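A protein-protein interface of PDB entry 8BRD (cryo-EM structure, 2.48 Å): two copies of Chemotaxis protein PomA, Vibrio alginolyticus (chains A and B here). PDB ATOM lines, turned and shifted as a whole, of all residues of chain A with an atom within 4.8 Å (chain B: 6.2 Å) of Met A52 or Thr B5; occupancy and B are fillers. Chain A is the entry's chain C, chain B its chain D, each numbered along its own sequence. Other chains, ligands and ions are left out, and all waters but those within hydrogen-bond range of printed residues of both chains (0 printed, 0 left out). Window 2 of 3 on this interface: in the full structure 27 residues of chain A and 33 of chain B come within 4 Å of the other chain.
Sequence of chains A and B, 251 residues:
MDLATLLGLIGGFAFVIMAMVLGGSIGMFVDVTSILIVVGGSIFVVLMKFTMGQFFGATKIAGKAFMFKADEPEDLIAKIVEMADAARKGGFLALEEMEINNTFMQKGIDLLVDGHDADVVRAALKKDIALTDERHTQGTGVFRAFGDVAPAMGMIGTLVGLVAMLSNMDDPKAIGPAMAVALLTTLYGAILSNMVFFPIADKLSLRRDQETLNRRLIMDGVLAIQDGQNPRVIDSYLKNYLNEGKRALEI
Among the printed residues, pairs that only touch across the chains: Leu A47 with Thr B5 (3.6 Å), Leu A47 with Gly B8 (3.6 Å), Leu A47 with Leu B9 (3.9 Å), Phe A50 with Thr B5 (3.8 Å), Thr A51 with Asp B2 (3.2 Å), Thr A51 with Thr B5 (3.4 Å), Met A52 with Ala B4 (3.3 Å) and Met A52 with Gly B8 (3.8 Å).
Of chain B, only Ala B4, Thr B5 and Gly B8 come within 4 Å of Met A52. Thr B5 touches just these residues of chain A: Leu A47 (3.6 Å), Phe A50 (3.8 Å), Thr A51 (3.4 Å) and Met A52 (3.1 Å). Of the printed residues of chain B, Leu A47 touches Thr B5 (3.6 Å), Gly B8 (3.6 Å) and Leu B9 (3.9 Å). Of the printed residues of chain A, Asp B2 touches Thr A51. Leu B7 touches none of the printed residues of chain A. The nearest printed residue of chain A that does not touch Leu B9 is Met A52 (5.9 Å).
No position is printed for both chains. Of the 9 pairs that touch across the chains among the printed residues, none has its exchanged pair printed and touching as well.
Of the 8 printed residues of chain A, 4 touch a printed residue of chain B. Among the printed residues, 9 pairs touch across the chains. Among the printed residues, no Asp or Glu carboxylate lies within 4 Å of a Lys or Arg side-chain nitrogen of the other chain.
The backbone NH (N) of Met A52 lies within hydrogen-bond range of the side-chain hydroxyl (OG1) of Thr B5 (3.1 Å).
OG1 of Thr B5 is in hydrogen-bond range of OD2 of Asp B2, 3.0 Å away. The backbone NH of Gln A54 is in hydrogen-bond range of the side-chain hydroxyl of Thr A51.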
ATOM      1  N   LEU A  47      14.831   7.902 -12.661  1.00  0.00           N
ATOM      2  CA  LEU A  47      14.724   7.143 -11.424  1.00  0.00           C
ATOM      3  C   LEU A  47      15.721   5.997 -11.339  1.00  0.00           C
ATOM      4  O   LEU A  47      15.917   5.454 -10.250  1.00  0.00           O
ATOM      5  CB  LEU A  47      13.303   6.609 -11.261  1.00  0.00           C
ATOM      6  CG  LEU A  47      12.304   7.646 -10.752  1.00  0.00           C
ATOM      7  CD1 LEU A  47      10.928   7.044 -10.667  1.00  0.00           C
ATOM      8  CD2 LEU A  47      12.743   8.183  -9.403  1.00  0.00           C
ATOM      9  N   PHE A  50      18.214   8.770  -9.841  1.00  0.00           N
ATOM     10  CA  PHE A  50      17.771   9.507  -8.670  1.00  0.00           C
ATOM     11  C   PHE A  50      16.666   8.730  -7.974  1.00  0.00           C
ATOM     12  O   PHE A  50      16.001   7.883  -8.571  1.00  0.00           O
ATOM     13  CB  PHE A  50      17.268  10.909  -9.039  1.00  0.00           C
ATOM     14  CG  PHE A  50      18.281  11.753  -9.754  1.00  0.00           C
ATOM     15  CD1 PHE A  50      19.150  12.561  -9.046  1.00  0.00           C
ATOM     16  CD2 PHE A  50      18.361  11.743 -11.133  1.00  0.00           C
ATOM     17  CE1 PHE A  50      20.080  13.338  -9.701  1.00  0.00           C
ATOM     18  CE2 PHE A  50      19.289  12.515 -11.790  1.00  0.00           C
ATOM     19  CZ  PHE A  50      20.149  13.314 -11.075  1.00  0.00           C
ATOM     20  N   THR A  51      16.483   9.019  -6.693  1.00  0.00           N
ATOM     21  CA  THR A  51      15.401   8.410  -5.938  1.00  0.00           C
ATOM     22  C   THR A  51      14.096   9.163  -6.178  1.00  0.00           C
ATOM     23  O   THR A  51      14.075  10.271  -6.717  1.00  0.00           O
ATOM     24  CB  THR A  51      15.729   8.394  -4.448  1.00  0.00           C
ATOM     25  OG1 THR A  51      15.993   9.728  -4.003  1.00  0.00           O
ATOM     26  CG2 THR A  51      16.952   7.543  -4.192  1.00  0.00           C
ATOM     27  N   MET A  52      12.952   8.615  -5.836  1.00  0.00           N
ATOM     28  CA  MET A  52      11.670   9.343  -5.901  1.00  0.00           C
ATOM     29  C   MET A  52      11.728  10.516  -4.933  1.00  0.00           C
ATOM     30  O   MET A  52      11.147  11.520  -5.230  1.00  0.00           O
ATOM     31  CB  MET A  52      10.496   8.464  -5.514  1.00  0.00           C
ATOM     32  CG  MET A  52       9.806   7.845  -6.653  1.00  0.00           C
ATOM     33  SD  MET A  52       8.928   9.129  -7.489  1.00  0.00           S
ATOM     34  CE  MET A  52       7.864   8.132  -8.525  1.00  0.00           C
ATOM     35  N   GLY A  53      12.347  10.380  -3.780  1.00  0.00           N
ATOM     36  CA  GLY A  53      12.444  11.550  -2.923  1.00  0.00           C
ATOM     37  C   GLY A  53      13.209  12.680  -3.576  1.00  0.00           C
ATOM     38  O   GLY A  53      12.826  13.845  -3.475  1.00  0.00           O
ATOM     39  N   GLN A  54      14.306  12.348  -4.262  1.00  0.00           N
ATOM     40  CA  GLN A  54      15.068  13.364  -4.980  1.00  0.00           C
ATOM     41  C   GLN A  54      14.258  13.984  -6.110  1.00  0.00           C
ATOM     42  O   GLN A  54      14.323  15.199  -6.321  1.00  0.00           O
ATOM     43  CB  GLN A  54      16.361  12.760  -5.520  1.00  0.00           C
ATOM     44  CG  GLN A  54      17.574  13.046  -4.666  1.00  0.00           C
ATOM     45  CD  GLN A  54      18.660  12.009  -4.831  1.00  0.00           C
ATOM     46  OE1 GLN A  54      18.847  11.457  -5.911  1.00  0.00           O
ATOM     47  NE2 GLN A  54      19.383  11.732  -3.754  1.00  0.00           N
ATOM     48  N   PHE A  55      13.492  13.174  -6.843  1.00  0.00           N
ATOM     49  CA  PHE A  55      12.641  13.711  -7.898  1.00  0.00           C
ATOM     50  C   PHE A  55      11.572  14.640  -7.330  1.00  0.00           C
ATOM     51  O   PHE A  55      11.325  15.723  -7.876  1.00  0.00           O
ATOM     52  CB  PHE A  55      12.010  12.559  -8.681  1.00  0.00           C
ATOM     53  CG  PHE A  55      11.077  12.999  -9.765  1.00  0.00           C
ATOM     54  CD1 PHE A  55      11.367  14.102 -10.548  1.00  0.00           C
ATOM     55  CD2 PHE A  55       9.910  12.301 -10.012  1.00  0.00           C
ATOM     56  CE1 PHE A  55      10.507  14.506 -11.539  1.00  0.00           C
ATOM     57  CE2 PHE A  55       9.050  12.701 -11.010  1.00  0.00           C
ATOM     58  CZ  PHE A  55       9.351  13.804 -11.774  1.00  0.00           C
ATOM     59  N   PHE A  56      10.936  14.241  -6.228  1.00  0.00           N
ATOM     60  CA  PHE A  56       9.934  15.099  -5.603  1.00  0.00           C
ATOM     61  C   PHE A  56      10.555  16.391  -5.088  1.00  0.00           C
ATOM     62  O   PHE A  56       9.958  17.465  -5.216  1.00  0.00           O
ATOM     63  CB  PHE A  56       9.232  14.351  -4.472  1.00  0.00           C
ATOM     64  CG  PHE A  56       8.202  13.369  -4.944  1.00  0.00           C
ATOM     65  CD1 PHE A  56       7.520  13.578  -6.129  1.00  0.00           C
ATOM     66  CD2 PHE A  56       7.924  12.230  -4.209  1.00  0.00           C
ATOM     67  CE1 PHE A  56       6.575  12.673  -6.570  1.00  0.00           C
ATOM     68  CE2 PHE A  56       6.978  11.323  -4.645  1.00  0.00           C
ATOM     69  CZ  PHE A  56       6.303  11.545  -5.827  1.00  0.00           C
ATOM     70  N   MET B   1      17.017  -0.671  -3.331  1.00  0.00           N
ATOM     71  CA  MET B   1      16.616   0.730  -3.357  1.00  0.00           C
ATOM     72  C   MET B   1      15.322   0.936  -2.582  1.00  0.00           C
ATOM     73  O   MET B   1      14.749  -0.014  -2.048  1.00  0.00           O
ATOM     74  CB  MET B   1      16.449   1.214  -4.796  1.00  0.00           C
ATOM     75  CG  MET B   1      15.556   0.331  -5.642  1.00  0.00           C
ATOM     76  SD  MET B   1      15.142   1.097  -7.216  1.00  0.00           S
ATOM     77  CE  MET B   1      16.776   1.444  -7.859  1.00  0.00           C
ATOM     78  N   ASP B   2      14.865   2.184  -2.523  1.00  0.00           N
ATOM     79  CA  ASP B   2      13.658   2.507  -1.779  1.00  0.00           C
ATOM     80  C   ASP B   2      12.430   1.937  -2.476  1.00  0.00           C
ATOM     81  O   ASP B   2      12.419   1.721  -3.689  1.00  0.00           O
ATOM     82  CB  ASP B   2      13.516   4.021  -1.630  1.00  0.00           C
ATOM     83  CG  ASP B   2      14.850   4.719  -1.500  1.00  0.00           C
ATOM     84  OD1 ASP B   2      15.577   4.443  -0.522  1.00  0.00           O
ATOM     85  OD2 ASP B   2      15.173   5.541  -2.382  1.00  0.00           O
ATOM     86  N   LEU B   3      11.386   1.683  -1.684  1.00  0.00           N
ATOM     87  CA  LEU B   3      10.140   1.175  -2.251  1.00  0.00           C
ATOM     88  C   LEU B   3       9.518   2.184  -3.205  1.00  0.00           C
ATOM     89  O   LEU B   3       9.009   1.810  -4.264  1.00  0.00           O
ATOM     90  CB  LEU B   3       9.161   0.814  -1.136  1.00  0.00           C
ATOM     91  CG  LEU B   3       7.833   0.191  -1.579  1.00  0.00           C
ATOM     92  CD1 LEU B   3       8.062  -0.950  -2.558  1.00  0.00           C
ATOM     93  CD2 LEU B   3       7.037  -0.285  -0.377  1.00  0.00           C
ATOM     94  N   ALA B   4       9.542   3.471  -2.843  1.00  0.00           N
ATOM     95  CA  ALA B   4       8.982   4.494  -3.721  1.00  0.00           C
ATOM     96  C   ALA B   4       9.742   4.572  -5.039  1.00  0.00           C
ATOM     97  O   ALA B   4       9.131   4.667  -6.108  1.00  0.00           O
ATOM     98  CB  ALA B   4       8.991   5.849  -3.017  1.00  0.00           C
ATOM     99  N   THR B   5      11.075   4.525  -4.979  1.00  0.00           N
ATOM    100  CA  THR B   5      11.872   4.553  -6.200  1.00  0.00           C
ATOM    101  C   THR B   5      11.598   3.331  -7.066  1.00  0.00           C
ATOM    102  O   THR B   5      11.500   3.439  -8.292  1.00  0.00           O
ATOM    103  CB  THR B   5      13.358   4.639  -5.861  1.00  0.00           C
ATOM    104  OG1 THR B   5      13.573   5.694  -4.917  1.00  0.00           O
ATOM    105  CG2 THR B   5      14.172   4.911  -7.114  1.00  0.00           C
ATOM    106  N   LEU B   6      11.476   2.157  -6.443  1.00  0.00           N
ATOM    107  CA  LEU B   6      11.189   0.942  -7.199  1.00  0.00           C
ATOM    108  C   LEU B   6       9.814   1.007  -7.854  1.00  0.00           C
ATOM    109  O   LEU B   6       9.650   0.594  -9.007  1.00  0.00           O
ATOM    110  CB  LEU B   6      11.297  -0.278  -6.288  1.00  0.00           C
ATOM    111  CG  LEU B   6      10.880  -1.616  -6.897  1.00  0.00           C
ATOM    112  CD1 LEU B   6      11.829  -2.007  -8.014  1.00  0.00           C
ATOM    113  CD2 LEU B   6      10.836  -2.691  -5.827  1.00  0.00           C
ATOM    114  N   LEU B   7       8.811   1.512  -7.130  1.00  0.00           N
ATOM    115  CA  LEU B   7       7.487   1.661  -7.721  1.00  0.00           C
ATOM    116  C   LEU B   7       7.507   2.654  -8.871  1.00  0.00           C
ATOM    117  O   LEU B   7       6.832   2.448  -9.883  1.00  0.00           O
ATOM    118  CB  LEU B   7       6.469   2.082  -6.662  1.00  0.00           C
ATOM    119  CG  LEU B   7       6.256   1.122  -5.491  1.00  0.00           C
ATOM    120  CD1 LEU B   7       5.371   1.761  -4.435  1.00  0.00           C
ATOM    121  CD2 LEU B   7       5.661  -0.189  -5.974  1.00  0.00           C
ATOM    122  N   GLY B   8       8.273   3.737  -8.741  1.00  0.00           N
ATOM    123  CA  GLY B   8       8.416   4.660  -9.856  1.00  0.00           C
ATOM    124  C   GLY B   8       9.085   4.023 -11.060  1.00  0.00           C
ATOM    125  O   GLY B   8       8.697   4.275 -12.204  1.00  0.00           O
ATOM    126  N   LEU B   9      10.102   3.192 -10.819  1.00  0.00           N
ATOM    127  CA  LEU B   9      10.766   2.483 -11.909  1.00  0.00           C
ATOM    128  C   LEU B   9       9.799   1.551 -12.624  1.00  0.00           C
ATOM    129  O   LEU B   9       9.736   1.523 -13.860  1.00  0.00           O
ATOM    130  CB  LEU B   9      11.958   1.695 -11.367  1.00  0.00           C
ATOM    131  CG  LEU B   9      13.312   2.396 -11.344  1.00  0.00           C
ATOM    132  CD1 LEU B   9      14.341   1.515 -10.677  1.00  0.00           C
ATOM    133  CD2 LEU B   9      13.742   2.725 -12.749  1.00  0.00           C
ATOM    134  N   ILE B  10       9.032   0.779 -11.854  1.00  0.00           N
ATOM    135  CA  ILE B  10       8.061  -0.133 -12.449  1.00  0.00           C
ATOM    136  C   ILE B  10       6.970   0.644 -13.167  1.00  0.00           C
ATOM    137  O   ILE B  10       6.478   0.211 -14.211  1.00  0.00           O
ATOM    138  CB  ILE B  10       7.480  -1.076 -11.378  1.00  0.00           C
ATOM    139  CG1 ILE B  10       8.605  -1.825 -10.662  1.00  0.00           C
ATOM    140  CG2 ILE B  10       6.514  -2.067 -12.002  1.00  0.00           C
ATOM    141  CD1 ILE B  10       9.565  -2.532 -11.592  1.00  0.00           C
